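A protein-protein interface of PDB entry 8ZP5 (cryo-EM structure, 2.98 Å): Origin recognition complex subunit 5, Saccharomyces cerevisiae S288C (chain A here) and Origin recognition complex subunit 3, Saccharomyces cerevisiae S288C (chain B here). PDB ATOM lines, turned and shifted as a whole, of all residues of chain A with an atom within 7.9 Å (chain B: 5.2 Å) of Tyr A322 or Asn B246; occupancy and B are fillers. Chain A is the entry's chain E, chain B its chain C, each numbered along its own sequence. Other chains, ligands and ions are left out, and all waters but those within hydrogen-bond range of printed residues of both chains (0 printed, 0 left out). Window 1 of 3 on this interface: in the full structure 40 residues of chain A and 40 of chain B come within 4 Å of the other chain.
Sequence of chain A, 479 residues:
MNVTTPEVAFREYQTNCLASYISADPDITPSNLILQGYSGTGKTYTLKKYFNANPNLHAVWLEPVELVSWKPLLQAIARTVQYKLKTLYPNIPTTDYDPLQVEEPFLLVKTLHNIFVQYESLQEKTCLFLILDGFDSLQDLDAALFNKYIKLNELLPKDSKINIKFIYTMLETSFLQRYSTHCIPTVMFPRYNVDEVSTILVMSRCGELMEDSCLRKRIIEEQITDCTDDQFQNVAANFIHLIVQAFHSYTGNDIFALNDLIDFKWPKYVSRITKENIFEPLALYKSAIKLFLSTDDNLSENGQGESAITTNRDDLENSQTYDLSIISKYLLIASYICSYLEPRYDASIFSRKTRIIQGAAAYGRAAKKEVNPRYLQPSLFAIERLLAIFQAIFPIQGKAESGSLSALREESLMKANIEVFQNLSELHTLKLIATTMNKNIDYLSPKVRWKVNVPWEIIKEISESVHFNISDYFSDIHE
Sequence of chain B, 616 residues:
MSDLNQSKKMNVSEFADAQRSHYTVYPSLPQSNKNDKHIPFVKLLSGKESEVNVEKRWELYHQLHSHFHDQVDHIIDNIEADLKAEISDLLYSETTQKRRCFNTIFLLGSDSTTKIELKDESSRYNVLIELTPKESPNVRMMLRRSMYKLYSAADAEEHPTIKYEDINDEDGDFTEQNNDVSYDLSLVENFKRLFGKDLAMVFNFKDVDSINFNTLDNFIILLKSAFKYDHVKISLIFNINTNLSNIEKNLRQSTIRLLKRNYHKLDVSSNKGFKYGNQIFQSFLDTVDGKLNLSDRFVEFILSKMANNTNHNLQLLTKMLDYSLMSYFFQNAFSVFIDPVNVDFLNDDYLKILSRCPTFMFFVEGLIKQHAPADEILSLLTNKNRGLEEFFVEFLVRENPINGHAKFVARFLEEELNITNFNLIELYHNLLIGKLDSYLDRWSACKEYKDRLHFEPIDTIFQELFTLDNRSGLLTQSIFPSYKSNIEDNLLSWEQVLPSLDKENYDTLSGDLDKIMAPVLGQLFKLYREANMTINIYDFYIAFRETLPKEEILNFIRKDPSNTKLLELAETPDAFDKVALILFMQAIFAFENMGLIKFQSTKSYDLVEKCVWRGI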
ATOM      1  N   GLN A 320      23.563 -28.959 -14.530  1.00  0.00           N
ATOM      2  CA  GLN A 320      22.903 -28.021 -15.428  1.00  0.00           C
ATOM      3  C   GLN A 320      23.013 -26.592 -14.905  1.00  0.00           C
ATOM      4  O   GLN A 320      22.083 -25.799 -15.043  1.00  0.00           O
ATOM      5  CB  GLN A 320      21.433 -28.400 -15.616  1.00  0.00           C
ATOM      6  N   THR A 321      24.158 -26.272 -14.299  1.00  0.00           N
ATOM      7  CA  THR A 321      24.369 -24.923 -13.786  1.00  0.00           C
ATOM      8  C   THR A 321      24.489 -23.908 -14.916  1.00  0.00           C
ATOM      9  O   THR A 321      24.081 -22.752 -14.755  1.00  0.00           O
ATOM     10  CB  THR A 321      25.617 -24.883 -12.902  1.00  0.00           C
ATOM     11  OG1 THR A 321      25.568 -25.958 -11.957  1.00  0.00           O
ATOM     12  CG2 THR A 321      25.690 -23.565 -12.143  1.00  0.00           C
ATOM     13  N   TYR A 322      25.038 -24.313 -16.058  1.00  0.00           N
ATOM     14  CA  TYR A 322      25.175 -23.436 -17.209  1.00  0.00           C
ATOM     15  C   TYR A 322      24.698 -24.155 -18.461  1.00  0.00           C
ATOM     16  O   TYR A 322      24.754 -25.385 -18.553  1.00  0.00           O
ATOM     17  CB  TYR A 322      26.626 -22.975 -17.405  1.00  0.00           C
ATOM     18  CG  TYR A 322      27.185 -22.172 -16.255  1.00  0.00           C
ATOM     19  CD1 TYR A 322      27.746 -22.799 -15.153  1.00  0.00           C
ATOM     20  CD2 TYR A 322      27.156 -20.785 -16.274  1.00  0.00           C
ATOM     21  CE1 TYR A 322      28.261 -22.069 -14.101  1.00  0.00           C
ATOM     22  CE2 TYR A 322      27.668 -20.047 -15.226  1.00  0.00           C
ATOM     23  CZ  TYR A 322      28.219 -20.694 -14.143  1.00  0.00           C
ATOM     24  OH  TYR A 322      28.730 -19.963 -13.095  1.00  0.00           O
ATOM     25  N   ASP A 323      24.226 -23.370 -19.426  1.00  0.00           N
ATOM     26  CA  ASP A 323      23.826 -23.874 -20.738  1.00  0.00           C
ATOM     27  C   ASP A 323      24.923 -23.655 -21.769  1.00  0.00           C
ATOM     28  O   ASP A 323      24.650 -23.397 -22.943  1.00  0.00           O
ATOM     29  CB  ASP A 323      22.524 -23.217 -21.189  1.00  0.00           C
ATOM     30  CG  ASP A 323      21.327 -23.684 -20.384  1.00  0.00           C
ATOM     31  OD1 ASP A 323      21.367 -24.817 -19.858  1.00  0.00           O
ATOM     32  OD2 ASP A 323      20.344 -22.920 -20.280  1.00  0.00           O
ATOM     33  N   LEU A 324      26.178 -23.753 -21.339  1.00  0.00           N
ATOM     34  CA  LEU A 324      27.312 -23.478 -22.204  1.00  0.00           C
ATOM     35  C   LEU A 324      27.467 -24.565 -23.265  1.00  0.00           C
ATOM     36  O   LEU A 324      26.932 -25.670 -23.149  1.00  0.00           O
ATOM     37  CB  LEU A 324      28.594 -23.375 -21.380  1.00  0.00           C
ATOM     38  CG  LEU A 324      28.686 -22.204 -20.402  1.00  0.00           C
ATOM     39  CD1 LEU A 324      29.944 -22.315 -19.562  1.00  0.00           C
ATOM     40  CD2 LEU A 324      28.651 -20.880 -21.144  1.00  0.00           C
ATOM     41  N   SER A 325      28.217 -24.231 -24.310  1.00  0.00           N
ATOM     42  CA  SER A 325      28.515 -25.180 -25.368  1.00  0.00           C
ATOM     43  C   SER A 325      29.589 -26.161 -24.907  1.00  0.00           C
ATOM     44  O   SER A 325      30.217 -25.993 -23.860  1.00  0.00           O
ATOM     45  CB  SER A 325      28.968 -24.448 -26.628  1.00  0.00           C
ATOM     46  OG  SER A 325      30.064 -23.595 -26.351  1.00  0.00           O
ATOM     47  N   SER A 328      32.830 -24.367 -24.805  1.00  0.00           N
ATOM     48  CA  SER A 328      32.941 -23.527 -23.616  1.00  0.00           C
ATOM     49  C   SER A 328      33.137 -24.365 -22.359  1.00  0.00           C
ATOM     50  O   SER A 328      33.913 -23.992 -21.470  1.00  0.00           O
ATOM     51  CB  SER A 328      31.704 -22.640 -23.484  1.00  0.00           C
ATOM     52  OG  SER A 328      31.759 -21.866 -22.301  1.00  0.00           O
ATOM     53  N   LYS A 329      32.440 -25.499 -22.261  1.00  0.00           N
ATOM     54  CA  LYS A 329      32.612 -26.372 -21.105  1.00  0.00           C
ATOM     55  C   LYS A 329      34.033 -26.919 -21.036  1.00  0.00           C
ATOM     56  O   LYS A 329      34.651 -26.930 -19.965  1.00  0.00           O
ATOM     57  CB  LYS A 329      31.597 -27.512 -21.152  1.00  0.00           C
ATOM     58  CG  LYS A 329      30.193 -27.105 -20.740  1.00  0.00           C
ATOM     59  CD  LYS A 329      29.187 -28.199 -21.050  1.00  0.00           C
ATOM     60  CE  LYS A 329      27.811 -27.853 -20.507  1.00  0.00           C
ATOM     61  NZ  LYS A 329      26.753 -28.718 -21.096  1.00  0.00           N
ATOM     62  N   LEU A 332      36.381 -24.167 -19.922  1.00  0.00           N
ATOM     63  CA  LEU A 332      36.353 -23.991 -18.472  1.00  0.00           C
ATOM     64  C   LEU A 332      37.104 -25.110 -17.764  1.00  0.00           C
ATOM     65  O   LEU A 332      37.825 -24.865 -16.790  1.00  0.00           O
ATOM     66  CB  LEU A 332      34.912 -23.915 -17.971  1.00  0.00           C
ATOM     67  CG  LEU A 332      34.322 -22.514 -17.828  1.00  0.00           C
ATOM     68  CD1 LEU A 332      32.871 -22.597 -17.401  1.00  0.00           C
ATOM     69  CD2 LEU A 332      35.127 -21.700 -16.831  1.00  0.00           C
ATOM     70  N   LEU A 427      33.361 -16.512 -22.259  1.00  0.00           N
ATOM     71  CA  LEU A 427      33.606 -16.986 -20.902  1.00  0.00           C
ATOM     72  C   LEU A 427      34.170 -15.874 -20.034  1.00  0.00           C
ATOM     73  O   LEU A 427      33.773 -15.719 -18.873  1.00  0.00           O
ATOM     74  CB  LEU A 427      34.561 -18.178 -20.925  1.00  0.00           C
ATOM     75  CG  LEU A 427      33.935 -19.561 -21.082  1.00  0.00           C
ATOM     76  CD1 LEU A 427      35.008 -20.631 -21.021  1.00  0.00           C
ATOM     77  CD2 LEU A 427      32.885 -19.788 -20.013  1.00  0.00           C
ATOM     78  N   LEU A 430      31.206 -13.458 -19.232  1.00  0.00           N
ATOM     79  CA  LEU A 430      30.335 -13.934 -18.164  1.00  0.00           C
ATOM     80  C   LEU A 430      31.030 -13.992 -16.811  1.00  0.00           C
ATOM     81  O   LEU A 430      30.449 -14.522 -15.857  1.00  0.00           O
ATOM     82  CB  LEU A 430      29.776 -15.316 -18.512  1.00  0.00           C
ATOM     83  CG  LEU A 430      29.192 -15.487 -19.913  1.00  0.00           C
ATOM     84  CD1 LEU A 430      28.903 -16.951 -20.197  1.00  0.00           C
ATOM     85  CD2 LEU A 430      27.937 -14.650 -20.069  1.00  0.00           C
ATOM     86  N   LYS A 431      32.256 -13.478 -16.713  1.00  0.00           N
ATOM     87  CA  LYS A 431      33.055 -13.419 -15.492  1.00  0.00           C
ATOM     88  C   LYS A 431      33.416 -14.794 -14.950  1.00  0.00           C
ATOM     89  O   LYS A 431      33.845 -14.901 -13.795  1.00  0.00           O
ATOM     90  CB  LYS A 431      32.358 -12.605 -14.395  1.00  0.00           C
ATOM     91  CG  LYS A 431      31.850 -11.251 -14.858  1.00  0.00           C
ATOM     92  CD  LYS A 431      32.909 -10.176 -14.683  1.00  0.00           C
ATOM     93  CE  LYS A 431      32.410  -8.827 -15.168  1.00  0.00           C
ATOM     94  NZ  LYS A 431      32.625  -8.655 -16.632  1.00  0.00           N
ATOM     95  N   LEU A 432      33.255 -15.854 -15.745  1.00  0.00           N
ATOM     96  CA  LEU A 432      33.686 -17.176 -15.301  1.00  0.00           C
ATOM     97  C   LEU A 432      35.205 -17.288 -15.325  1.00  0.00           C
ATOM     98  O   LEU A 432      35.792 -18.040 -14.538  1.00  0.00           O
ATOM     99  CB  LEU A 432      33.045 -18.256 -16.169  1.00  0.00           C
ATOM    100  CG  LEU A 432      31.516 -18.262 -16.168  1.00  0.00           C
ATOM    101  CD1 LEU A 432      30.975 -19.488 -16.879  1.00  0.00           C
ATOM    102  CD2 LEU A 432      30.985 -18.190 -14.747  1.00  0.00           C
ATOM    103  N   ASN A 453      37.156 -18.253 -12.170  1.00  0.00           N
ATOM    104  CA  ASN A 453      36.201 -17.757 -11.179  1.00  0.00           C
ATOM    105  C   ASN A 453      35.015 -18.701 -11.044  1.00  0.00           C
ATOM    106  O   ASN A 453      33.856 -18.281 -11.028  1.00  0.00           O
ATOM    107  CB  ASN A 453      35.690 -16.360 -11.509  1.00  0.00           C
ATOM    108  CG  ASN A 453      36.737 -15.296 -11.316  1.00  0.00           C
ATOM    109  OD1 ASN A 453      36.846 -14.374 -12.116  1.00  0.00           O
ATOM    110  ND2 ASN A 453      37.515 -15.413 -10.247  1.00  0.00           N
ATOM    111  N   VAL A 454      35.280 -19.998 -10.945  1.00  0.00           N
ATOM    112  CA  VAL A 454      34.219 -20.945 -10.612  1.00  0.00           C
ATOM    113  C   VAL A 454      34.666 -21.761  -9.407  1.00  0.00           C
ATOM    114  O   VAL A 454      35.866 -22.037  -9.253  1.00  0.00           O
ATOM    115  CB  VAL A 454      33.856 -21.847 -11.805  1.00  0.00           C
ATOM    116  CG1 VAL A 454      33.472 -21.011 -13.015  1.00  0.00           C
ATOM    117  CG2 VAL A 454      34.989 -22.802 -12.140  1.00  0.00           C
ATOM    118  N   PRO A 455      33.758 -22.144  -8.521  1.00  0.00           N
ATOM    119  CA  PRO A 455      34.120 -23.010  -7.398  1.00  0.00           C
ATOM    120  C   PRO A 455      34.311 -24.443  -7.882  1.00  0.00           C
ATOM    121  O   PRO A 455      34.138 -24.759  -9.057  1.00  0.00           O
ATOM    122  CB  PRO A 455      32.922 -22.881  -6.457  1.00  0.00           C
ATOM    123  CG  PRO A 455      31.783 -22.539  -7.350  1.00  0.00           C
ATOM    124  CD  PRO A 455      32.359 -21.692  -8.445  1.00  0.00           C
ATOM    125  N   ILE A 458      30.930 -26.212  -9.275  1.00  0.00           N
ATOM    126  CA  ILE A 458      30.493 -25.858 -10.622  1.00  0.00           C
ATOM    127  C   ILE A 458      31.340 -26.574 -11.666  1.00  0.00           C
ATOM    128  O   ILE A 458      30.817 -27.137 -12.637  1.00  0.00           O
ATOM    129  CB  ILE A 458      30.530 -24.330 -10.811  1.00  0.00           C
ATOM    130  CG1 ILE A 458      29.288 -23.690 -10.190  1.00  0.00           C
ATOM    131  CG2 ILE A 458      30.642 -23.971 -12.283  1.00  0.00           C
ATOM    132  CD1 ILE A 458      29.262 -22.183 -10.289  1.00  0.00           C
ATOM    133  N   ILE A 459      32.663 -26.571 -11.481  1.00  0.00           N
ATOM    134  CA  ILE A 459      33.529 -27.232 -12.451  1.00  0.00           C
ATOM    135  C   ILE A 459      33.346 -28.744 -12.397  1.00  0.00           C
ATOM    136  O   ILE A 459      33.460 -29.422 -13.423  1.00  0.00           O
ATOM    137  CB  ILE A 459      34.998 -26.816 -12.242  1.00  0.00           C
ATOM    138  CG1 ILE A 459      35.809 -27.092 -13.508  1.00  0.00           C
ATOM    139  CG2 ILE A 459      35.613 -27.523 -11.047  1.00  0.00           C
ATOM    140  CD1 ILE A 459      35.408 -26.236 -14.686  1.00  0.00           C
ATOM    141  N   GLU A 461      30.442 -30.260 -11.753  1.00  0.00           N
ATOM    142  CA  GLU A 461      29.210 -30.497 -12.500  1.00  0.00           C
ATOM    143  C   GLU A 461      29.445 -30.375 -14.000  1.00  0.00           C
ATOM    144  O   GLU A 461      28.925 -31.175 -14.786  1.00  0.00           O
ATOM    145  CB  GLU A 461      28.126 -29.523 -12.042  1.00  0.00           C
ATOM    146  CG  GLU A 461      26.833 -29.620 -12.834  1.00  0.00           C
ATOM    147  CD  GLU A 461      25.650 -29.038 -12.087  1.00  0.00           C
ATOM    148  OE1 GLU A 461      25.867 -28.190 -11.196  1.00  0.00           O
ATOM    149  OE2 GLU A 461      24.503 -29.429 -12.391  1.00  0.00           O
ATOM    150  N   ILE A 462      30.231 -29.379 -14.415  1.00  0.00           N
ATOM    151  CA  ILE A 462      30.531 -29.215 -15.835  1.00  0.00           C
ATOM    152  C   ILE A 462      31.307 -30.416 -16.361  1.00  0.00           C
ATOM    153  O   ILE A 462      31.021 -30.932 -17.449  1.00  0.00           O
ATOM    154  CB  ILE A 462      31.291 -27.895 -16.069  1.00  0.00           C
ATOM    155  CG1 ILE A 462      30.307 -26.726 -16.138  1.00  0.00           C
ATOM    156  CG2 ILE A 462      32.121 -27.964 -17.340  1.00  0.00           C
ATOM    157  CD1 ILE A 462      30.956 -25.376 -15.976  1.00  0.00           C
ATOM    158  N   SER A 465      29.130 -33.301 -16.760  1.00  0.00           N
ATOM    159  CA  SER A 465      28.191 -33.104 -17.860  1.00  0.00           C
ATOM    160  C   SER A 465      28.755 -33.631 -19.174  1.00  0.00           C
ATOM    161  O   SER A 465      28.037 -34.267 -19.953  1.00  0.00           O
ATOM    162  CB  SER A 465      27.833 -31.624 -17.985  1.00  0.00           C
ATOM    163  OG  SER A 465      26.980 -31.398 -19.093  1.00  0.00           O
ATOM    164  N   PHE B 213      27.786  -7.673  -7.441  1.00  0.00           N
ATOM    165  CA  PHE B 213      26.710  -8.153  -6.588  1.00  0.00           C
ATOM    166  C   PHE B 213      26.708  -7.501  -5.215  1.00  0.00           C
ATOM    167  O   PHE B 213      25.670  -7.506  -4.548  1.00  0.00           O
ATOM    168  CB  PHE B 213      26.791  -9.672  -6.455  1.00  0.00           C
ATOM    169  CG  PHE B 213      26.261 -10.405  -7.651  1.00  0.00           C
ATOM    170  CD1 PHE B 213      24.899 -10.515  -7.862  1.00  0.00           C
ATOM    171  CD2 PHE B 213      27.125 -10.970  -8.572  1.00  0.00           C
ATOM    172  CE1 PHE B 213      24.407 -11.183  -8.963  1.00  0.00           C
ATOM    173  CE2 PHE B 213      26.638 -11.641  -9.675  1.00  0.00           C
ATOM    174  CZ  PHE B 213      25.277 -11.746  -9.871  1.00  0.00           C
ATOM    175  N   THR B 242      22.712 -16.959 -16.795  1.00  0.00           N
ATOM    176  CA  THR B 242      23.106 -18.259 -16.267  1.00  0.00           C
ATOM    177  C   THR B 242      21.977 -18.835 -15.422  1.00  0.00           C
ATOM    178  O   THR B 242      20.842 -18.354 -15.488  1.00  0.00           O
ATOM    179  CB  THR B 242      24.384 -18.152 -15.431  1.00  0.00           C
ATOM    180  OG1 THR B 242      24.102 -17.454 -14.211  1.00  0.00           O
ATOM    181  CG2 THR B 242      25.472 -17.410 -16.196  1.00  0.00           C
ATOM    182  N   ASN B 243      22.254 -19.893 -14.669  1.00  0.00           N
ATOM    183  CA  ASN B 243      21.312 -20.302 -13.641  1.00  0.00           C
ATOM    184  C   ASN B 243      21.360 -19.315 -12.477  1.00  0.00           C
ATOM    185  O   ASN B 243      22.295 -18.522 -12.339  1.00  0.00           O
ATOM    186  CB  ASN B 243      21.619 -21.715 -13.149  1.00  0.00           C
ATOM    187  CG  ASN B 243      20.418 -22.384 -12.509  1.00  0.00           C
ATOM    188  OD1 ASN B 243      19.275 -21.996 -12.751  1.00  0.00           O
ATOM    189  ND2 ASN B 243      20.670 -23.397 -11.688  1.00  0.00           N
ATOM    190  N   LEU B 244      20.333 -19.368 -11.633  1.00  0.00           N
ATOM    191  CA  LEU B 244      20.251 -18.454 -10.501  1.00  0.00           C
ATOM    192  C   LEU B 244      21.105 -18.894  -9.319  1.00  0.00           C
ATOM    193  O   LEU B 244      21.165 -18.171  -8.319  1.00  0.00           O
ATOM    194  CB  LEU B 244      18.789 -18.275 -10.070  1.00  0.00           C
ATOM    195  CG  LEU B 244      17.950 -19.458  -9.579  1.00  0.00           C
ATOM    196  CD1 LEU B 244      18.177 -19.762  -8.103  1.00  0.00           C
ATOM    197  CD2 LEU B 244      16.479 -19.187  -9.845  1.00  0.00           C
ATOM    198  N   SER B 245      21.759 -20.056  -9.405  1.00  0.00           N
ATOM    199  CA  SER B 245      22.633 -20.495  -8.323  1.00  0.00           C
ATOM    200  C   SER B 245      23.808 -19.546  -8.129  1.00  0.00           C
ATOM    201  O   SER B 245      24.264 -19.349  -6.998  1.00  0.00           O
ATOM    202  CB  SER B 245      23.134 -21.914  -8.594  1.00  0.00           C
ATOM    203  OG  SER B 245      22.103 -22.864  -8.389  1.00  0.00           O
ATOM    204  N   ASN B 246      24.315 -18.957  -9.215  1.00  0.00           N
ATOM    205  CA  ASN B 246      25.384 -17.972  -9.086  1.00  0.00           C
ATOM    206  C   ASN B 246      24.923 -16.768  -8.275  1.00  0.00           C
ATOM    207  O   ASN B 246      25.667 -16.256  -7.430  1.00  0.00           O
ATOM    208  CB  ASN B 246      25.863 -17.532 -10.469  1.00  0.00           C
ATOM    209  CG  ASN B 246      26.602 -18.627 -11.205  1.00  0.00           C
ATOM    210  OD1 ASN B 246      27.380 -19.373 -10.612  1.00  0.00           O
ATOM    211  ND2 ASN B 246      26.362 -18.731 -12.507  1.00  0.00           N
ATOM    212  N   ILE B 247      23.697 -16.305  -8.517  1.00  0.00           N
ATOM    213  CA  ILE B 247      23.157 -15.192  -7.745  1.00  0.00           C
ATOM    214  C   ILE B 247      22.955 -15.596  -6.290  1.00  0.00           C
ATOM    215  O   ILE B 247      23.200 -14.803  -5.374  1.00  0.00           O
ATOM    216  CB  ILE B 247      21.857 -14.683  -8.392  1.00  0.00           C
ATOM    217  CG1 ILE B 247      22.180 -13.927  -9.679  1.00  0.00           C
ATOM    218  CG2 ILE B 247      21.075 -13.805  -7.440  1.00  0.00           C
ATOM    219  CD1 ILE B 247      20.968 -13.454 -10.412  1.00  0.00           C
ATOM    220  N   GLU B 248      22.516 -16.834  -6.051  1.00  0.00           N
ATOM    221  CA  GLU B 248      22.379 -17.312  -4.679  1.00  0.00           C
ATOM    222  C   GLU B 248      23.719 -17.301  -3.958  1.00  0.00           C
ATOM    223  O   GLU B 248      23.802 -16.910  -2.788  1.00  0.00           O
ATOM    224  CB  GLU B 248      21.781 -18.718  -4.667  1.00  0.00           C
ATOM    225  CG  GLU B 248      20.289 -18.767  -4.932  1.00  0.00           C
ATOM    226  CD  GLU B 248      19.693 -20.126  -4.627  1.00  0.00           C
ATOM    227  OE1 GLU B 248      20.466 -21.062  -4.336  1.00  0.00           O
ATOM    228  OE2 GLU B 248      18.453 -20.260  -4.678  1.00  0.00           O
ATOM    229  N   LYS B 249      24.782 -17.732  -4.639  1.00  0.00           N
ATOM    230  CA  LYS B 249      26.106 -17.719  -4.027  1.00  0.00           C
ATOM    231  C   LYS B 249      26.630 -16.301  -3.838  1.00  0.00           C
ATOM    232  O   LYS B 249      27.375 -16.041  -2.887  1.00  0.00           O
ATOM    233  CB  LYS B 249      27.085 -18.532  -4.873  1.00  0.00           C
ATOM    234  CG  LYS B 249      27.295 -19.958  -4.393  1.00  0.00           C
ATOM    235  CD  LYS B 249      26.203 -20.880  -4.907  1.00  0.00           C
ATOM    236  CE  LYS B 249      26.490 -22.330  -4.556  1.00  0.00           C
ATOM    237  NZ  LYS B 249      25.248 -23.153  -4.551  1.00  0.00           N
ATOM    238  N   ASN B 250      26.260 -15.377  -4.723  1.00  0.00           N
ATOM    239  CA  ASN B 250      26.795 -14.023  -4.702  1.00  0.00           C
ATOM    240  C   ASN B 250      25.951 -13.043  -3.897  1.00  0.00           C
ATOM    241  O   ASN B 250      26.340 -11.878  -3.768  1.00  0.00           O
ATOM    242  CB  ASN B 250      26.955 -13.502  -6.133  1.00  0.00           C
ATOM    243  CG  ASN B 250      27.970 -14.294  -6.931  1.00  0.00           C
ATOM    244  OD1 ASN B 250      29.007 -14.701  -6.408  1.00  0.00           O
ATOM    245  ND2 ASN B 250      27.675 -14.520  -8.205  1.00  0.00           N
ATOM    246  N   LEU B 251      24.816 -13.471  -3.354  1.00  0.00           N
ATOM    247  CA  LEU B 251      23.974 -12.609  -2.539  1.00  0.00           C
ATOM    248  C   LEU B 251      23.960 -13.085  -1.094  1.00  0.00           C
ATOM    249  O   LEU B 251      24.135 -14.274  -0.810  1.00  0.00           O
ATOM    250  CB  LEU B 251      22.536 -12.555  -3.066  1.00  0.00           C
ATOM    251  CG  LEU B 251      22.250 -11.760  -4.338  1.00  0.00           C
ATOM    252  CD1 LEU B 251      20.755 -11.737  -4.599  1.00  0.00           C
ATOM    253  CD2 LEU B 251      22.798 -10.349  -4.234  1.00  0.00           C
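ND2 of Asn B246 sits at hydrogen-bond distance from OG1 of Thr B242, at 3.1 Å. The side-chain amide nitrogen (ND2) of Asn B250 lies within hydrogen-bond range of the backbone carbonyl oxygen (O) of Asn B246 (2.8 Å).
Thr B242 touches Tyr A322. Ile A458 touches Asn B246.
OH of Tyr A322 sits at hydrogen-bond distance from ND2 of Asn B246 (2.7 Å). The backbone NH (N) of Asn B243 lies close to the backbone carbonyl oxygen (O) of Thr A321, at 3.4 Å.
Gln A320 touches none of the printed residues of chain B. Printed residues of chain B within 4 Å of Thr A321: Asn B243 (3.1 Å). Tyr A322 touches just these residues of chain B: Thr B242 (3.6 Å) and Asn B246 (2.7 Å). Printed residues of chain B within 4 Å of Ile A458: Asn B246 (3.4 Å). Of the printed residues of chain A, Thr B242 touches Tyr A322 (3.6 Å). Printed residues of chain A within 4 Å of Asn B243: Thr A321. Printed residues of chain A within 4 Å of Asn B246: Tyr A322 and Ile A458. The nearest printed residue of chain B that does not touch Tyr A322 is Asn B243 (5.2 Å). The nearest residue of chain A that does not touch Asn B246 is Thr A321 (4.8 Å). The nearest printed residue of chain A that does not touch Asn B243 is Gln A320 (4.4 Å).
Of the 21 printed residues of chain A, 3 touch a printed residue of chain B.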
